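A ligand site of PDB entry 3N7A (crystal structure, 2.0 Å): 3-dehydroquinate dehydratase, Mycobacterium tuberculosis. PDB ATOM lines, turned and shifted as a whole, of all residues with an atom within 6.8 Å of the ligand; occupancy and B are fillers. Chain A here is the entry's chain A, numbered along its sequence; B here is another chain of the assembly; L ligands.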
ATOM      1  N   PRO A  12     -25.945   4.661  10.883  1.00  0.00           N
ATOM      2  CA  PRO A  12     -25.959   3.235  10.598  1.00  0.00           C
ATOM      3  C   PRO A  12     -25.455   2.910   9.252  1.00  0.00           C
ATOM      4  O   PRO A  12     -25.676   3.715   8.333  1.00  0.00           O
ATOM      5  CB  PRO A  12     -27.468   2.886  10.673  1.00  0.00           C
ATOM      6  CG  PRO A  12     -27.966   3.846  11.731  1.00  0.00           C
ATOM      7  CD  PRO A  12     -27.229   5.121  11.421  1.00  0.00           C
ATOM      8  N   ASN A  13     -24.751   1.778   9.181  1.00  0.00           N
ATOM      9  CA  ASN A  13     -24.133   1.089   7.985  1.00  0.00           C
ATOM     10  C   ASN A  13     -22.900   1.834   7.513  1.00  0.00           C
ATOM     11  O   ASN A  13     -22.110   1.283   6.806  1.00  0.00           O
ATOM     12  CB  ASN A  13     -25.172   0.794   6.869  1.00  0.00           C
ATOM     13  CG  ASN A  13     -26.430   0.123   7.467  1.00  0.00           C
ATOM     14  OD1 ASN A  13     -26.303  -0.825   8.238  1.00  0.00           O
ATOM     15  ND2 ASN A  13     -27.620   0.643   7.155  1.00  0.00           N
ATOM     16  N   LEU A  14     -22.689   3.048   7.989  1.00  0.00           N
ATOM     17  CA  LEU A  14     -21.592   3.832   7.401  1.00  0.00           C
ATOM     18  C   LEU A  14     -20.213   3.325   7.878  1.00  0.00           C
ATOM     19  O   LEU A  14     -19.175   3.680   7.315  1.00  0.00           O
ATOM     20  CB  LEU A  14     -21.796   5.342   7.587  1.00  0.00           C
ATOM     21  CG  LEU A  14     -22.935   5.899   6.737  1.00  0.00           C
ATOM     22  CD1 LEU A  14     -23.231   7.245   7.212  1.00  0.00           C
ATOM     23  CD2 LEU A  14     -22.653   5.925   5.237  1.00  0.00           C
ATOM     24  N   VAL A  24     -21.979   4.161  -5.762  1.00  0.00           N
ATOM     25  CA  VAL A  24     -22.902   4.927  -4.878  1.00  0.00           C
ATOM     26  C   VAL A  24     -22.218   5.786  -3.751  1.00  0.00           C
ATOM     27  O   VAL A  24     -22.482   7.008  -3.630  1.00  0.00           O
ATOM     28  CB  VAL A  24     -23.986   4.002  -4.201  1.00  0.00           C
ATOM     29  CG1 VAL A  24     -25.173   4.831  -3.698  1.00  0.00           C
ATOM     30  CG2 VAL A  24     -24.459   2.838  -5.129  1.00  0.00           C
ATOM     31  N   TYR A  25     -21.349   5.134  -2.951  1.00  0.00           N
ATOM     32  CA  TYR A  25     -20.766   5.689  -1.684  1.00  0.00           C
ATOM     33  C   TYR A  25     -19.199   5.893  -1.700  1.00  0.00           C
ATOM     34  O   TYR A  25     -18.617   6.302  -0.661  1.00  0.00           O
ATOM     35  CB  TYR A  25     -21.218   4.888  -0.421  1.00  0.00           C
ATOM     36  CG  TYR A  25     -22.733   4.764  -0.172  1.00  0.00           C
ATOM     37  CD1 TYR A  25     -23.431   3.609  -0.538  1.00  0.00           C
ATOM     38  CD2 TYR A  25     -23.469   5.814   0.400  1.00  0.00           C
ATOM     39  CE1 TYR A  25     -24.837   3.489  -0.342  1.00  0.00           C
ATOM     40  CE2 TYR A  25     -24.854   5.694   0.602  1.00  0.00           C
ATOM     41  CZ  TYR A  25     -25.522   4.552   0.217  1.00  0.00           C
ATOM     42  OH  TYR A  25     -26.886   4.440   0.454  1.00  0.00           O
ATOM     43  N   ASN A  76     -23.895  12.880   8.787  1.00  0.00           N
ATOM     44  CA  ASN A  76     -24.482  11.948   7.824  1.00  0.00           C
ATOM     45  C   ASN A  76     -25.254  10.894   8.657  1.00  0.00           C
ATOM     46  O   ASN A  76     -24.719   9.909   9.134  1.00  0.00           O
ATOM     47  CB  ASN A  76     -23.405  11.310   6.928  1.00  0.00           C
ATOM     48  CG  ASN A  76     -23.997  10.446   5.780  1.00  0.00           C
ATOM     49  OD1 ASN A  76     -25.171  10.031   5.844  1.00  0.00           O
ATOM     50  ND2 ASN A  76     -23.157  10.141   4.766  1.00  0.00           N
ATOM     51  N   ALA A  77     -26.541  11.156   8.865  1.00  0.00           N
ATOM     52  CA  ALA A  77     -27.363  10.240   9.618  1.00  0.00           C
ATOM     53  C   ALA A  77     -27.725   8.958   8.949  1.00  0.00           C
ATOM     54  O   ALA A  77     -28.345   8.111   9.583  1.00  0.00           O
ATOM     55  CB  ALA A  77     -28.648  10.942  10.221  1.00  0.00           C
ATOM     56  N   GLY A  78     -27.353   8.765   7.681  1.00  0.00           N
ATOM     57  CA  GLY A  78     -27.686   7.484   7.026  1.00  0.00           C
ATOM     58  C   GLY A  78     -29.219   7.392   6.939  1.00  0.00           C
ATOM     59  O   GLY A  78     -29.863   8.400   6.700  1.00  0.00           O
ATOM     60  N   GLY A  79     -29.769   6.189   7.099  1.00  0.00           N
ATOM     61  CA  GLY A  79     -31.211   5.943   7.082  1.00  0.00           C
ATOM     62  C   GLY A  79     -32.039   6.696   8.118  1.00  0.00           C
ATOM     63  O   GLY A  79     -33.202   6.911   7.917  1.00  0.00           O
ATOM     64  N   LEU A  80     -31.432   7.085   9.237  1.00  0.00           N
ATOM     65  CA  LEU A  80     -32.214   7.796  10.219  1.00  0.00           C
ATOM     66  C   LEU A  80     -32.606   9.196   9.766  1.00  0.00           C
ATOM     67  O   LEU A  80     -33.515   9.814  10.349  1.00  0.00           O
ATOM     68  CB  LEU A  80     -31.429   7.919  11.547  1.00  0.00           C
ATOM     69  CG  LEU A  80     -31.056   6.583  12.165  1.00  0.00           C
ATOM     70  CD1 LEU A  80     -30.220   6.785  13.423  1.00  0.00           C
ATOM     71  CD2 LEU A  80     -32.296   5.747  12.577  1.00  0.00           C
ATOM     72  N   THR A  81     -31.893   9.698   8.736  1.00  0.00           N
ATOM     73  CA  THR A  81     -32.236  10.980   8.157  1.00  0.00           C
ATOM     74  C   THR A  81     -33.738  11.026   7.849  1.00  0.00           C
ATOM     75  O   THR A  81     -34.361  12.055   8.018  1.00  0.00           O
ATOM     76  CB  THR A  81     -31.534  11.122   6.781  1.00  0.00           C
ATOM     77  OG1 THR A  81     -30.099  11.009   6.926  1.00  0.00           O
ATOM     78  CG2 THR A  81     -31.937  12.432   6.141  1.00  0.00           C
ATOM     79  N   HIS A  82     -34.288   9.905   7.367  1.00  0.00           N
ATOM     80  CA  HIS A  82     -35.617   9.892   6.691  1.00  0.00           C
ATOM     81  C   HIS A  82     -36.684   9.467   7.692  1.00  0.00           C
ATOM     82  O   HIS A  82     -37.836   9.454   7.370  1.00  0.00           O
ATOM     83  CB  HIS A  82     -35.645   8.950   5.431  1.00  0.00           C
ATOM     84  CG  HIS A  82     -34.449   9.095   4.517  1.00  0.00           C
ATOM     85  ND1 HIS A  82     -34.153  10.261   3.830  1.00  0.00           N
ATOM     86  CD2 HIS A  82     -33.440   8.226   4.236  1.00  0.00           C
ATOM     87  CE1 HIS A  82     -32.989  10.115   3.216  1.00  0.00           C
ATOM     88  NE2 HIS A  82     -32.541   8.895   3.456  1.00  0.00           N
ATOM     89  N   VAL A 101     -24.996  16.031   5.593  1.00  0.00           N
ATOM     90  CA  VAL A 101     -24.223  15.585   4.446  1.00  0.00           C
ATOM     91  C   VAL A 101     -24.661  14.219   3.989  1.00  0.00           C
ATOM     92  O   VAL A 101     -24.750  13.325   4.797  1.00  0.00           O
ATOM     93  CB  VAL A 101     -22.676  15.499   4.774  1.00  0.00           C
ATOM     94  CG1 VAL A 101     -21.928  14.775   3.640  1.00  0.00           C
ATOM     95  CG2 VAL A 101     -22.105  16.863   4.963  1.00  0.00           C
ATOM     96  N   HIS A 102     -24.896  14.066   2.697  1.00  0.00           N
ATOM     97  CA  HIS A 102     -25.135  12.750   2.127  1.00  0.00           C
ATOM     98  C   HIS A 102     -24.116  12.519   0.999  1.00  0.00           C
ATOM     99  O   HIS A 102     -23.972  13.369   0.100  1.00  0.00           O
ATOM    100  CB  HIS A 102     -26.590  12.629   1.603  1.00  0.00           C
ATOM    101  CG  HIS A 102     -27.627  12.807   2.689  1.00  0.00           C
ATOM    102  ND1 HIS A 102     -27.969  11.800   3.564  1.00  0.00           N
ATOM    103  CD2 HIS A 102     -28.335  13.892   3.078  1.00  0.00           C
ATOM    104  CE1 HIS A 102     -28.856  12.254   4.435  1.00  0.00           C
ATOM    105  NE2 HIS A 102     -29.100  13.523   4.148  1.00  0.00           N
ATOM    106  N   ILE A 103     -23.474  11.361   1.026  1.00  0.00           N
ATOM    107  CA  ILE A 103     -22.473  10.960   0.026  1.00  0.00           C
ATOM    108  C   ILE A 103     -23.101  10.826  -1.358  1.00  0.00           C
ATOM    109  O   ILE A 103     -22.630  11.421  -2.335  1.00  0.00           O
ATOM    110  CB  ILE A 103     -21.796   9.655   0.499  1.00  0.00           C
ATOM    111  CG1 ILE A 103     -20.990   9.943   1.856  1.00  0.00           C
ATOM    112  CG2 ILE A 103     -20.986   8.991  -0.595  1.00  0.00           C
ATOM    113  CD1 ILE A 103     -20.558   8.643   2.537  1.00  0.00           C
ATOM    114  N   SER A 104     -24.203  10.077  -1.427  1.00  0.00           N
ATOM    115  CA  SER A 104     -24.862   9.781  -2.701  1.00  0.00           C
ATOM    116  C   SER A 104     -25.831  10.956  -3.005  1.00  0.00           C
ATOM    117  O   SER A 104     -26.124  11.782  -2.143  1.00  0.00           O
ATOM    118  CB  SER A 104     -25.642   8.460  -2.584  1.00  0.00           C
ATOM    119  OG  SER A 104     -26.841   8.592  -1.757  1.00  0.00           O
ATOM    120  N   ASN A 105     -26.346  11.023  -4.216  1.00  0.00           N
ATOM    121  CA  ASN A 105     -27.389  12.001  -4.502  1.00  0.00           C
ATOM    122  C   ASN A 105     -28.796  11.418  -4.205  1.00  0.00           C
ATOM    123  O   ASN A 105     -29.457  10.806  -5.076  1.00  0.00           O
ATOM    124  CB  ASN A 105     -27.320  12.435  -5.944  1.00  0.00           C
ATOM    125  CG  ASN A 105     -28.284  13.584  -6.262  1.00  0.00           C
ATOM    126  OD1 ASN A 105     -29.294  13.820  -5.551  1.00  0.00           O
ATOM    127  ND2 ASN A 105     -28.007  14.283  -7.366  1.00  0.00           N
ATOM    128  N   VAL A 106     -29.243  11.641  -2.998  1.00  0.00           N
ATOM    129  CA  VAL A 106     -30.487  11.087  -2.526  1.00  0.00           C
ATOM    130  C   VAL A 106     -31.676  11.482  -3.436  1.00  0.00           C
ATOM    131  O   VAL A 106     -32.689  10.780  -3.430  1.00  0.00           O
ATOM    132  CB  VAL A 106     -30.769  11.471  -1.059  1.00  0.00           C
ATOM    133  CG1 VAL A 106     -29.607  10.953  -0.080  1.00  0.00           C
ATOM    134  CG2 VAL A 106     -30.916  12.964  -0.912  1.00  0.00           C
ATOM    135  N   ARG A 109     -32.492   8.899  -6.198  1.00  0.00           N
ATOM    136  CA  ARG A 109     -32.702   7.503  -5.779  1.00  0.00           C
ATOM    137  C   ARG A 109     -34.177   7.264  -5.546  1.00  0.00           C
ATOM    138  O   ARG A 109     -35.011   7.956  -6.174  1.00  0.00           O
ATOM    139  CB  ARG A 109     -31.796   7.194  -4.583  1.00  0.00           C
ATOM    140  CG  ARG A 109     -30.291   7.244  -5.039  1.00  0.00           C
ATOM    141  CD  ARG A 109     -29.401   7.078  -3.859  1.00  0.00           C
ATOM    142  NE  ARG A 109     -29.398   5.700  -3.388  1.00  0.00           N
ATOM    143  CZ  ARG A 109     -28.913   5.286  -2.215  1.00  0.00           C
ATOM    144  NH1 ARG A 109     -28.350   6.156  -1.359  1.00  0.00           N
ATOM    145  NH2 ARG A 109     -28.978   3.979  -1.907  1.00  0.00           N
ATOM    146  N   PHE A 112     -38.526   7.866  -1.177  1.00  0.00           N
ATOM    147  CA  PHE A 112     -38.490   8.061   0.251  1.00  0.00           C
ATOM    148  C   PHE A 112     -37.172   8.703   0.715  1.00  0.00           C
ATOM    149  O   PHE A 112     -37.158   9.345   1.721  1.00  0.00           O
ATOM    150  CB  PHE A 112     -38.764   6.746   1.008  1.00  0.00           C
ATOM    151  CG  PHE A 112     -37.682   5.690   0.822  1.00  0.00           C
ATOM    152  CD1 PHE A 112     -36.463   5.754   1.527  1.00  0.00           C
ATOM    153  CD2 PHE A 112     -37.943   4.564   0.044  1.00  0.00           C
ATOM    154  CE1 PHE A 112     -35.497   4.757   1.361  1.00  0.00           C
ATOM    155  CE2 PHE A 112     -37.006   3.568  -0.094  1.00  0.00           C
ATOM    156  CZ  PHE A 112     -35.767   3.675   0.554  1.00  0.00           C
ATOM    157  N   ARG A 113     -36.099   8.534  -0.032  1.00  0.00           N
ATOM    158  CA  ARG A 113     -34.848   9.252   0.253  1.00  0.00           C
ATOM    159  C   ARG A 113     -34.860  10.759   0.053  1.00  0.00           C
ATOM    160  O   ARG A 113     -33.883  11.455   0.420  1.00  0.00           O
ATOM    161  CB  ARG A 113     -33.638   8.636  -0.466  1.00  0.00           C
ATOM    162  CG  ARG A 113     -33.381   7.215  -0.087  1.00  0.00           C
ATOM    163  CD  ARG A 113     -32.066   6.707  -0.633  1.00  0.00           C
ATOM    164  NE  ARG A 113     -32.051   5.242  -0.735  1.00  0.00           N
ATOM    165  CZ  ARG A 113     -31.770   4.402   0.261  1.00  0.00           C
ATOM    166  NH1 ARG A 113     -31.457   4.870   1.506  1.00  0.00           N
ATOM    167  NH2 ARG A 113     -31.817   3.091   0.029  1.00  0.00           N
ATOM    168  N   GLY A 128     -24.680  14.244  -2.713  1.00  0.00           N
ATOM    169  CA  GLY A 128     -24.197  13.844  -4.036  1.00  0.00           C
ATOM    170  C   GLY A 128     -22.754  14.164  -4.457  1.00  0.00           C
ATOM    171  O   GLY A 128     -22.339  13.857  -5.572  1.00  0.00           O
ATOM    172  N   TYR A 134     -17.875  16.042   2.970  1.00  0.00           N
ATOM    173  CA  TYR A 134     -17.579  16.271   4.386  1.00  0.00           C
ATOM    174  C   TYR A 134     -16.512  17.372   4.529  1.00  0.00           C
ATOM    175  O   TYR A 134     -16.588  18.249   5.417  1.00  0.00           O
ATOM    176  CB  TYR A 134     -16.957  15.023   4.990  1.00  0.00           C
ATOM    177  CG  TYR A 134     -17.897  13.845   5.211  1.00  0.00           C
ATOM    178  CD1 TYR A 134     -18.038  12.817   4.246  1.00  0.00           C
ATOM    179  CD2 TYR A 134     -18.639  13.763   6.398  1.00  0.00           C
ATOM    180  CE1 TYR A 134     -18.876  11.681   4.498  1.00  0.00           C
ATOM    181  CE2 TYR A 134     -19.503  12.653   6.657  1.00  0.00           C
ATOM    182  CZ  TYR A 134     -19.575  11.618   5.723  1.00  0.00           C
ATOM    183  OH  TYR A 134     -20.440  10.588   6.068  1.00  0.00           O
ATOM    184  N   VAL B  85     -35.348   2.510   7.367  1.00  0.00           N
ATOM    185  CA  VAL B  85     -34.489   2.536   6.175  1.00  0.00           C
ATOM    186  C   VAL B  85     -33.131   1.905   6.453  1.00  0.00           C
ATOM    187  O   VAL B  85     -32.562   1.162   5.638  1.00  0.00           O
ATOM    188  CB  VAL B  85     -34.383   4.020   5.670  1.00  0.00           C
ATOM    189  CG1 VAL B  85     -33.477   4.169   4.446  1.00  0.00           C
ATOM    190  CG2 VAL B  85     -35.813   4.470   5.330  1.00  0.00           C
ATOM    191  N   ALA B  86     -32.626   2.125   7.671  1.00  0.00           N
ATOM    192  CA  ALA B  86     -31.318   1.586   8.024  1.00  0.00           C
ATOM    193  C   ALA B  86     -31.349   0.078   7.876  1.00  0.00           C
ATOM    194  O   ALA B  86     -30.397  -0.521   7.332  1.00  0.00           O
ATOM    195  CB  ALA B  86     -30.972   2.017   9.562  1.00  0.00           C
ATOM    196  N   ASP B  89     -31.481  -0.870   4.128  1.00  0.00           N
ATOM    197  CA  ASP B  89     -30.142  -0.739   3.478  1.00  0.00           C
ATOM    198  C   ASP B  89     -29.153  -1.828   3.829  1.00  0.00           C
ATOM    199  O   ASP B  89     -28.384  -2.248   2.999  1.00  0.00           O
ATOM    200  CB  ASP B  89     -29.536   0.640   3.729  1.00  0.00           C
ATOM    201  CG  ASP B  89     -30.312   1.725   3.029  1.00  0.00           C
ATOM    202  OD1 ASP B  89     -31.226   1.401   2.225  1.00  0.00           O
ATOM    203  OD2 ASP B  89     -30.096   2.872   3.326  1.00  0.00           O
HETATM  204  C1  LIG L   1     -28.220   8.293   2.119  1.00  0.00           C
HETATM  205  C2  LIG L   1     -29.263   7.539   2.919  1.00  0.00           C
HETATM  206  O1  LIG L   1     -30.538   7.562   2.239  1.00  0.00           O
HETATM  207  C3  LIG L   1     -28.791   6.100   3.139  1.00  0.00           C
HETATM  208  O2  LIG L   1     -29.686   5.517   4.056  1.00  0.00           O
HETATM  209  C4  LIG L   1     -27.385   6.080   3.700  1.00  0.00           C
HETATM  210  C5  LIG L   1     -26.525   7.164   3.524  1.00  0.00           C
HETATM  211  C6  LIG L   1     -25.687   8.632   1.922  1.00  0.00           C
HETATM  212  O3  LIG L   1     -26.016   9.182   0.661  1.00  0.00           O
HETATM  213  O4  LIG L   1     -26.905   9.398   3.950  1.00  0.00           O
HETATM  214  O5  LIG L   1     -24.636   9.283   2.599  1.00  0.00           O
HETATM  215  C7  LIG L   1     -26.865   8.384   2.882  1.00  0.00           C
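Tyr 25 touches the ligand (CE2 to C6, 3.3 Å). Gly 78 touches the ligand. Val 106 touches the ligand. Hydrophobic or aromatic side chains that line the ligand: Tyr 25, His 82, His 102, Ile 103 and Val 106. The nearest printed residue that does not touch the ligand is Val 85 of chain B (4.04 Å).
OD1 of Asp 89 of chain B lies within salt-bridge range of NH2 of Arg 113, 2.8 Å away. O of Val 101 sits close to OD1 of Asn 76, at 3.5 Å. ND2 of Asn 76 sits at hydrogen-bond distance from OH of Tyr 134, 3.0 Å away. NH1 of Arg 109 lies within hydrogen-bond range of OG of Ser 104 (2.9 Å). The side-chain hydroxyl of Tyr 25 is in hydrogen-bond range of the guanidinium group of Arg 109. O of His 102 sits at hydrogen-bond distance from N of Gly 128 (3.0 Å). The backbone carbonyl oxygen of Ser 104 is in hydrogen-bond range of the backbone NH of Gly 128 (2.9 Å). The side-chain amide oxygen (OD1) of Asn 76 is in hydrogen-bond range of the backbone NH (N) of Gly 78, at 3.1 Å.
An oxygen (O4) of the ligand is in hydrogen-bond range of the side-chain amide oxygen (OD1) of Asn 76, at 2.6 Å. N of Ser 104 lies within hydrogen-bond range of O3 of the ligand (2.9 Å). OG of Ser 104 lies within hydrogen-bond range of O3 of the ligand (2.6 Å). An oxygen (O4) of the ligand sits at hydrogen-bond distance from a ring nitrogen (ND1) of His 102 (2.7 Å). The backbone NH (N) of Ile 103 lies within hydrogen-bond range of an oxygen (O5) of the ligand. An oxygen (O1) of the ligand is in hydrogen-bond range of a ring nitrogen (NE2) of His 82 (2.7 Å). The guanidinium group (NH1) of Arg 113 is in hydrogen-bond range of an oxygen (O1) of the ligand (2.9 Å). An oxygen (O2) of the ligand lies within hydrogen-bond range of the side-chain carboxylate (OD2) of Asp 89 of chain B, at 2.8 Å. N of Gly 79 is in hydrogen-bond range of O2 of the ligand.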
